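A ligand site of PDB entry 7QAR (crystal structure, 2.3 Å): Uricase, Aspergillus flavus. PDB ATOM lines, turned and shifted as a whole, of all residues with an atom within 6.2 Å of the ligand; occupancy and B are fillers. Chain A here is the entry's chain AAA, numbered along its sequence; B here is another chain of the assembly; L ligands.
The backbone NH of Gln 229 sits close to the side-chain hydroxyl of Ser 227 (3.3 Å).
N of Asn 255 lies within hydrogen-bond range of O of Gly 287, 2.8 Å away.
The side-chain hydroxyl (OG) of Ser 225 lies within hydrogen-bond range of the backbone carbonyl oxygen (O) of Ser 227.
A ring nitrogen (NE2) of His 257 sits at hydrogen-bond distance from the side-chain amino group of Lys 11 of chain B (2.7 Å).
The side-chain hydroxyl of Thr 58 of chain B lies within hydrogen-bond range of the side-chain amino group of Lys 11 of chain B, at 3.3 Å.
CE1 of Phe 160 touches N1 of the ligand, at 3.0 Å.
Leu 171 touches the ligand.
CA of Ser 227 touches O1 of the ligand (3.6 Å).
CE1 of His 257 touches O4 of the ligand (3.5 Å).
CA of Gly 287 touches O4 of the ligand, at 3.7 Å.
Ile 289 touches the ligand (CD1 to O3, 3.5 Å).
Ile 55 of chain B touches the ligand.
CB of Ala 57 of chain B touches O5 of the ligand, 3.5 Å away.
Hydrophobic or aromatic side chains within 4 Å of the ligand: Phe 160, Leu 171, Val 228, His 257, Ile 289, Ile 55 of chain B and Ala 57 of chain B.
Within 4 Å of the ligand: Phe 160, Leu 171, Arg 177, Ser 227, Val 228, Gln 229, Asn 255, His 257, Gly 287, Ile 289, Ile 55 of chain B, Ala 57 of chain B, Thr 58 of chain B and Asp 59 of chain B.
The nearest printed residue that does not touch the ligand is Tyr 9 of chain B (4.1 Å).
NH2 of Arg 177 sits at hydrogen-bond distance from O1 of the ligand (2.8 Å).
N of Asp 59 of chain B sits at hydrogen-bond distance from O5 of the ligand.
The backbone NH (N) of Val 228 is in hydrogen-bond range of an oxygen (O1) of the ligand (3.0 Å).
O5 of the ligand is in hydrogen-bond range of N of Thr 58 of chain B.
The side-chain hydroxyl (OG1) of Thr 58 of chain B lies within hydrogen-bond range of an oxygen (O4) of the ligand, 2.9 Å away.
The side-chain amide nitrogen (NE2) of Gln 229 is in hydrogen-bond range of an oxygen (O2) of the ligand, 3.0 Å away.
ND2 of Asn 255 is in hydrogen-bond range of O4 of the ligand, 2.8 Å away.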
ATOM      1  N   GLN A 159       5.361 -12.722  26.013  1.00  0.00           N
ATOM      2  CA  GLN A 159       4.589 -11.674  25.315  1.00  0.00           C
ATOM      3  C   GLN A 159       3.533 -12.319  24.436  1.00  0.00           C
ATOM      4  O   GLN A 159       3.681 -13.483  24.008  1.00  0.00           O
ATOM      5  CB  GLN A 159       5.484 -10.836  24.414  1.00  0.00           C
ATOM      6  CG  GLN A 159       6.618 -10.103  25.129  1.00  0.00           C
ATOM      7  CD  GLN A 159       7.507  -9.365  24.150  1.00  0.00           C
ATOM      8  OE1 GLN A 159       7.432  -8.150  24.008  1.00  0.00           O
ATOM      9  NE2 GLN A 159       8.348 -10.120  23.447  1.00  0.00           N
ATOM     10  N   PHE A 160       2.512 -11.543  24.094  1.00  0.00           N
ATOM     11  CA  PHE A 160       1.564 -11.970  23.048  1.00  0.00           C
ATOM     12  C   PHE A 160       0.852 -10.762  22.469  1.00  0.00           C
ATOM     13  O   PHE A 160      -0.094 -10.247  23.067  1.00  0.00           O
ATOM     14  CB  PHE A 160       0.574 -13.005  23.570  1.00  0.00           C
ATOM     15  CG  PHE A 160      -0.165 -13.711  22.472  1.00  0.00           C
ATOM     16  CD1 PHE A 160       0.495 -14.565  21.607  1.00  0.00           C
ATOM     17  CD2 PHE A 160      -1.531 -13.516  22.280  1.00  0.00           C
ATOM     18  CE1 PHE A 160      -0.179 -15.202  20.583  1.00  0.00           C
ATOM     19  CE2 PHE A 160      -2.202 -14.163  21.258  1.00  0.00           C
ATOM     20  CZ  PHE A 160      -1.536 -15.012  20.413  1.00  0.00           C
ATOM     21  N   LEU A 171      -9.352  -9.794  23.421  1.00  0.00           N
ATOM     22  CA  LEU A 171      -8.048  -9.914  24.115  1.00  0.00           C
ATOM     23  C   LEU A 171      -7.140  -8.707  23.870  1.00  0.00           C
ATOM     24  O   LEU A 171      -6.919  -8.319  22.698  1.00  0.00           O
ATOM     25  CB  LEU A 171      -7.358 -11.212  23.664  1.00  0.00           C
ATOM     26  CG  LEU A 171      -6.006 -11.507  24.312  1.00  0.00           C
ATOM     27  CD1 LEU A 171      -6.173 -11.946  25.760  1.00  0.00           C
ATOM     28  CD2 LEU A 171      -5.239 -12.555  23.518  1.00  0.00           C
ATOM     29  N   ARG A 177       3.507 -11.057  30.327  1.00  0.00           N
ATOM     30  CA  ARG A 177       2.557 -11.986  30.974  1.00  0.00           C
ATOM     31  C   ARG A 177       3.286 -13.134  31.629  1.00  0.00           C
ATOM     32  O   ARG A 177       4.484 -13.388  31.367  1.00  0.00           O
ATOM     33  CB  ARG A 177       1.506 -12.488  29.972  1.00  0.00           C
ATOM     34  CG  ARG A 177       2.082 -13.273  28.802  1.00  0.00           C
ATOM     35  CD  ARG A 177       1.024 -14.015  28.011  1.00  0.00           C
ATOM     36  NE  ARG A 177       1.656 -15.011  27.142  1.00  0.00           N
ATOM     37  CZ  ARG A 177       1.037 -15.706  26.188  1.00  0.00           C
ATOM     38  NH1 ARG A 177      -0.255 -15.535  25.961  1.00  0.00           N
ATOM     39  NH2 ARG A 177       1.720 -16.570  25.462  1.00  0.00           N
ATOM     40  N   LEU A 179       3.593 -17.172  31.751  1.00  0.00           N
ATOM     41  CA  LEU A 179       3.403 -18.343  30.889  1.00  0.00           C
ATOM     42  C   LEU A 179       3.559 -19.602  31.732  1.00  0.00           C
ATOM     43  O   LEU A 179       4.619 -19.779  32.338  1.00  0.00           O
ATOM     44  CB  LEU A 179       4.462 -18.301  29.784  1.00  0.00           C
ATOM     45  CG  LEU A 179       4.401 -19.419  28.743  1.00  0.00           C
ATOM     46  CD1 LEU A 179       3.092 -19.358  27.964  1.00  0.00           C
ATOM     47  CD2 LEU A 179       5.592 -19.339  27.800  1.00  0.00           C
ATOM     48  N   SER A 225       9.563 -14.986  25.092  1.00  0.00           N
ATOM     49  CA  SER A 225       8.620 -15.713  24.206  1.00  0.00           C
ATOM     50  C   SER A 225       7.675 -14.774  23.451  1.00  0.00           C
ATOM     51  O   SER A 225       6.929 -14.024  24.080  1.00  0.00           O
ATOM     52  CB  SER A 225       7.816 -16.732  24.987  1.00  0.00           C
ATOM     53  OG  SER A 225       6.896 -17.414  24.150  1.00  0.00           O
ATOM     54  N   ALA A 226       7.628 -14.926  22.128  1.00  0.00           N
ATOM     55  CA  ALA A 226       6.684 -14.193  21.272  1.00  0.00           C
ATOM     56  C   ALA A 226       5.313 -14.830  21.301  1.00  0.00           C
ATOM     57  O   ALA A 226       4.324 -14.143  20.948  1.00  0.00           O
ATOM     58  CB  ALA A 226       7.226 -14.147  19.873  1.00  0.00           C
ATOM     59  N   SER A 227       5.272 -16.123  21.639  1.00  0.00           N
ATOM     60  CA  SER A 227       4.074 -16.972  21.672  1.00  0.00           C
ATOM     61  C   SER A 227       4.496 -18.369  22.061  1.00  0.00           C
ATOM     62  O   SER A 227       5.692 -18.726  21.970  1.00  0.00           O
ATOM     63  CB  SER A 227       3.337 -16.971  20.361  1.00  0.00           C
ATOM     64  OG  SER A 227       4.035 -17.760  19.421  1.00  0.00           O
ATOM     65  N   VAL A 228       3.520 -19.164  22.467  1.00  0.00           N
ATOM     66  CA  VAL A 228       3.789 -20.619  22.713  1.00  0.00           C
ATOM     67  C   VAL A 228       4.306 -21.252  21.426  1.00  0.00           C
ATOM     68  O   VAL A 228       5.279 -22.032  21.472  1.00  0.00           O
ATOM     69  CB  VAL A 228       2.542 -21.352  23.243  1.00  0.00           C
ATOM     70  CG1 VAL A 228       2.883 -22.780  23.664  1.00  0.00           C
ATOM     71  CG2 VAL A 228       1.904 -20.611  24.409  1.00  0.00           C
ATOM     72  N   GLN A 229       3.680 -20.921  20.311  1.00  0.00           N
ATOM     73  CA  GLN A 229       4.054 -21.454  18.992  1.00  0.00           C
ATOM     74  C   GLN A 229       5.550 -21.251  18.735  1.00  0.00           C
ATOM     75  O   GLN A 229       6.266 -22.201  18.338  1.00  0.00           O
ATOM     76  CB  GLN A 229       3.211 -20.786  17.908  1.00  0.00           C
ATOM     77  CG  GLN A 229       1.752 -21.233  17.881  1.00  0.00           C
ATOM     78  CD  GLN A 229       0.841 -20.450  18.803  1.00  0.00           C
ATOM     79  OE1 GLN A 229       1.258 -19.917  19.827  1.00  0.00           O
ATOM     80  NE2 GLN A 229      -0.436 -20.403  18.455  1.00  0.00           N
ATOM     81  N   ASN A 255      -1.925 -23.718  27.288  1.00  0.00           N
ATOM     82  CA  ASN A 255      -1.665 -22.352  27.792  1.00  0.00           C
ATOM     83  C   ASN A 255      -2.549 -22.149  29.016  1.00  0.00           C
ATOM     84  O   ASN A 255      -3.750 -21.983  28.879  1.00  0.00           O
ATOM     85  CB  ASN A 255      -1.871 -21.323  26.677  1.00  0.00           C
ATOM     86  CG  ASN A 255      -1.353 -19.927  27.009  1.00  0.00           C
ATOM     87  OD1 ASN A 255      -0.704 -19.721  28.034  1.00  0.00           O
ATOM     88  ND2 ASN A 255      -1.639 -18.981  26.138  1.00  0.00           N
ATOM     89  N   HIS A 257      -3.854 -20.158  31.652  1.00  0.00           N
ATOM     90  CA  HIS A 257      -4.009 -18.695  31.806  1.00  0.00           C
ATOM     91  C   HIS A 257      -3.977 -18.260  33.268  1.00  0.00           C
ATOM     92  O   HIS A 257      -4.615 -18.878  34.120  1.00  0.00           O
ATOM     93  CB  HIS A 257      -5.297 -18.213  31.141  1.00  0.00           C
ATOM     94  CG  HIS A 257      -5.343 -18.505  29.686  1.00  0.00           C
ATOM     95  ND1 HIS A 257      -4.262 -18.290  28.856  1.00  0.00           N
ATOM     96  CD2 HIS A 257      -6.333 -19.012  28.912  1.00  0.00           C
ATOM     97  CE1 HIS A 257      -4.578 -18.635  27.626  1.00  0.00           C
ATOM     98  NE2 HIS A 257      -5.846 -19.078  27.634  1.00  0.00           N
ATOM     99  N   ASN A 286      -8.572 -23.493  28.504  1.00  0.00           N
ATOM    100  CA  ASN A 286      -7.105 -23.372  28.286  1.00  0.00           C
ATOM    101  C   ASN A 286      -6.822 -23.406  26.800  1.00  0.00           C
ATOM    102  O   ASN A 286      -7.355 -24.274  26.095  1.00  0.00           O
ATOM    103  CB  ASN A 286      -6.333 -24.460  29.042  1.00  0.00           C
ATOM    104  CG  ASN A 286      -6.843 -25.860  28.733  1.00  0.00           C
ATOM    105  OD1 ASN A 286      -7.850 -26.301  29.283  1.00  0.00           O
ATOM    106  ND2 ASN A 286      -6.152 -26.566  27.850  1.00  0.00           N
ATOM    107  N   GLY A 287      -5.918 -22.541  26.350  1.00  0.00           N
ATOM    108  CA  GLY A 287      -5.275 -22.725  25.047  1.00  0.00           C
ATOM    109  C   GLY A 287      -4.670 -24.097  24.942  1.00  0.00           C
ATOM    110  O   GLY A 287      -4.183 -24.614  25.947  1.00  0.00           O
ATOM    111  N   LEU A 288      -4.621 -24.645  23.730  1.00  0.00           N
ATOM    112  CA  LEU A 288      -3.919 -25.910  23.430  1.00  0.00           C
ATOM    113  C   LEU A 288      -3.215 -25.714  22.100  1.00  0.00           C
ATOM    114  O   LEU A 288      -3.893 -25.496  21.096  1.00  0.00           O
ATOM    115  CB  LEU A 288      -4.937 -27.049  23.336  1.00  0.00           C
ATOM    116  CG  LEU A 288      -4.354 -28.424  23.031  1.00  0.00           C
ATOM    117  CD1 LEU A 288      -3.247 -28.785  24.025  1.00  0.00           C
ATOM    118  CD2 LEU A 288      -5.438 -29.490  23.057  1.00  0.00           C
ATOM    119  N   ILE A 289      -1.875 -25.754  22.150  1.00  0.00           N
ATOM    120  CA  ILE A 289      -0.978 -25.431  21.001  1.00  0.00           C
ATOM    121  C   ILE A 289      -0.215 -26.712  20.664  1.00  0.00           C
ATOM    122  O   ILE A 289       0.462 -27.246  21.543  1.00  0.00           O
ATOM    123  CB  ILE A 289      -0.032 -24.262  21.324  1.00  0.00           C
ATOM    124  CG1 ILE A 289      -0.683 -23.178  22.186  1.00  0.00           C
ATOM    125  CG2 ILE A 289       0.547 -23.696  20.047  1.00  0.00           C
ATOM    126  CD1 ILE A 289      -1.883 -22.508  21.539  1.00  0.00           C
ATOM    127  N   TYR B   9      -4.098 -25.783  16.616  1.00  0.00           N
ATOM    128  CA  TYR B   9      -4.114 -24.995  17.858  1.00  0.00           C
ATOM    129  C   TYR B   9      -5.525 -24.478  18.091  1.00  0.00           C
ATOM    130  O   TYR B   9      -6.291 -24.277  17.145  1.00  0.00           O
ATOM    131  CB  TYR B   9      -3.092 -23.856  17.788  1.00  0.00           C
ATOM    132  CG  TYR B   9      -3.667 -22.621  17.149  1.00  0.00           C
ATOM    133  CD1 TYR B   9      -3.849 -22.561  15.778  1.00  0.00           C
ATOM    134  CD2 TYR B   9      -4.132 -21.560  17.915  1.00  0.00           C
ATOM    135  CE1 TYR B   9      -4.429 -21.465  15.180  1.00  0.00           C
ATOM    136  CE2 TYR B   9      -4.716 -20.453  17.325  1.00  0.00           C
ATOM    137  CZ  TYR B   9      -4.873 -20.409  15.951  1.00  0.00           C
ATOM    138  OH  TYR B   9      -5.449 -19.332  15.357  1.00  0.00           O
ATOM    139  N   GLY B  10      -5.853 -24.180  19.331  1.00  0.00           N
ATOM    140  CA  GLY B  10      -7.185 -23.693  19.645  1.00  0.00           C
ATOM    141  C   GLY B  10      -7.453 -23.679  21.126  1.00  0.00           C
ATOM    142  O   GLY B  10      -6.510 -23.670  21.949  1.00  0.00           O
ATOM    143  N   LYS B  11      -8.748 -23.671  21.450  1.00  0.00           N
ATOM    144  CA  LYS B  11      -9.207 -23.586  22.854  1.00  0.00           C
ATOM    145  C   LYS B  11      -9.850 -24.909  23.239  1.00  0.00           C
ATOM    146  O   LYS B  11     -10.743 -25.400  22.552  1.00  0.00           O
ATOM    147  CB  LYS B  11     -10.164 -22.411  23.058  1.00  0.00           C
ATOM    148  CG  LYS B  11     -10.432 -22.068  24.519  1.00  0.00           C
ATOM    149  CD  LYS B  11      -9.223 -21.552  25.271  1.00  0.00           C
ATOM    150  CE  LYS B  11      -9.045 -20.053  25.152  1.00  0.00           C
ATOM    151  NZ  LYS B  11      -8.027 -19.549  26.097  1.00  0.00           N
ATOM    152  N   ASN B  52       2.634 -13.484  14.602  1.00  0.00           N
ATOM    153  CA  ASN B  52       1.332 -13.645  15.300  1.00  0.00           C
ATOM    154  C   ASN B  52       0.178 -13.198  14.419  1.00  0.00           C
ATOM    155  O   ASN B  52      -0.973 -13.461  14.750  1.00  0.00           O
ATOM    156  CB  ASN B  52       1.345 -12.923  16.652  1.00  0.00           C
ATOM    157  CG  ASN B  52       2.254 -13.602  17.658  1.00  0.00           C
ATOM    158  OD1 ASN B  52       2.635 -14.765  17.478  1.00  0.00           O
ATOM    159  ND2 ASN B  52       2.607 -12.908  18.727  1.00  0.00           N
ATOM    160  N   ILE B  55      -2.521 -15.644  13.577  1.00  0.00           N
ATOM    161  CA  ILE B  55      -3.149 -16.360  14.724  1.00  0.00           C
ATOM    162  C   ILE B  55      -4.478 -15.690  15.072  1.00  0.00           C
ATOM    163  O   ILE B  55      -4.474 -14.522  15.518  1.00  0.00           O
ATOM    164  CB  ILE B  55      -2.190 -16.441  15.924  1.00  0.00           C
ATOM    165  CG1 ILE B  55      -0.917 -17.235  15.586  1.00  0.00           C
ATOM    166  CG2 ILE B  55      -2.903 -17.023  17.148  1.00  0.00           C
ATOM    167  CD1 ILE B  55      -1.170 -18.656  15.112  1.00  0.00           C
ATOM    168  N   VAL B  56      -5.561 -16.436  14.874  1.00  0.00           N
ATOM    169  CA  VAL B  56      -6.890 -16.161  15.489  1.00  0.00           C
ATOM    170  C   VAL B  56      -6.737 -16.554  16.947  1.00  0.00           C
ATOM    171  O   VAL B  56      -6.573 -17.728  17.254  1.00  0.00           O
ATOM    172  CB  VAL B  56      -8.008 -16.979  14.801  1.00  0.00           C
ATOM    173  CG1 VAL B  56      -9.360 -16.770  15.473  1.00  0.00           C
ATOM    174  CG2 VAL B  56      -8.081 -16.689  13.321  1.00  0.00           C
ATOM    175  N   ALA B  57      -6.733 -15.597  17.858  1.00  0.00           N
ATOM    176  CA  ALA B  57      -6.374 -15.898  19.249  1.00  0.00           C
ATOM    177  C   ALA B  57      -7.326 -16.947  19.821  1.00  0.00           C
ATOM    178  O   ALA B  57      -8.531 -16.962  19.506  1.00  0.00           O
ATOM    179  CB  ALA B  57      -6.375 -14.638  20.070  1.00  0.00           C
ATOM    180  N   THR B  58      -6.781 -17.853  20.630  1.00  0.00           N
ATOM    181  CA  THR B  58      -7.663 -18.851  21.280  1.00  0.00           C
ATOM    182  C   THR B  58      -8.742 -18.149  22.122  1.00  0.00           C
ATOM    183  O   THR B  58      -9.880 -18.648  22.184  1.00  0.00           O
ATOM    184  CB  THR B  58      -6.885 -19.900  22.073  1.00  0.00           C
ATOM    185  OG1 THR B  58      -6.352 -19.293  23.251  1.00  0.00           O
ATOM    186  CG2 THR B  58      -5.799 -20.565  21.257  1.00  0.00           C
ATOM    187  N   ASP B  59      -8.420 -16.996  22.692  1.00  0.00           N
ATOM    188  CA  ASP B  59      -9.440 -16.201  23.417  1.00  0.00           C
ATOM    189  C   ASP B  59     -10.610 -15.839  22.494  1.00  0.00           C
ATOM    190  O   ASP B  59     -11.783 -15.882  22.910  1.00  0.00           O
ATOM    191  CB  ASP B  59      -8.874 -14.919  24.022  1.00  0.00           C
ATOM    192  CG  ASP B  59      -9.829 -14.258  25.007  1.00  0.00           C
ATOM    193  OD1 ASP B  59     -10.026 -14.834  26.100  1.00  0.00           O
ATOM    194  OD2 ASP B  59     -10.416 -13.208  24.662  1.00  0.00           O
ATOM    195  N   SER B  60     -10.296 -15.488  21.242  1.00  0.00           N
ATOM    196  CA  SER B  60     -11.321 -15.190  20.212  1.00  0.00           C
ATOM    197  C   SER B  60     -12.108 -16.421  19.826  1.00  0.00           C
ATOM    198  O   SER B  60     -13.306 -16.313  19.555  1.00  0.00           O
ATOM    199  CB  SER B  60     -10.668 -14.543  19.008  1.00  0.00           C
ATOM    200  OG  SER B  60      -9.810 -13.483  19.394  1.00  0.00           O
HETATM  201  O1  LIG L   1       0.899 -17.848  23.162  1.00  0.00           O
HETATM  202  C1  LIG L   1      -0.248 -17.656  22.836  1.00  0.00           C
HETATM  203  N1  LIG L   1      -0.628 -18.019  21.577  1.00  0.00           N
HETATM  204  C2  LIG L   1      -1.901 -18.376  21.282  1.00  0.00           C
HETATM  205  O2  LIG L   1      -2.247 -18.706  20.157  1.00  0.00           O
HETATM  206  N2  LIG L   1      -1.083 -17.092  23.725  1.00  0.00           N
HETATM  207  C3  LIG L   1      -2.351 -17.285  23.415  1.00  0.00           C
HETATM  208  N3  LIG L   1      -3.420 -16.543  23.862  1.00  0.00           N
HETATM  209  C4  LIG L   1      -3.363 -15.474  24.869  1.00  0.00           C
HETATM  210  C5  LIG L   1      -2.898 -18.306  22.423  1.00  0.00           C
HETATM  211  O3  LIG L   1      -3.174 -19.617  22.967  1.00  0.00           O
HETATM  212  O4  LIG L   1      -3.702 -19.479  24.340  1.00  0.00           O
HETATM  213  N4  LIG L   1      -4.109 -17.620  22.029  1.00  0.00           N
HETATM  214  C6  LIG L   1      -4.502 -16.767  22.985  1.00  0.00           C
HETATM  215  O5  LIG L   1      -5.598 -16.230  23.098  1.00  0.00           O
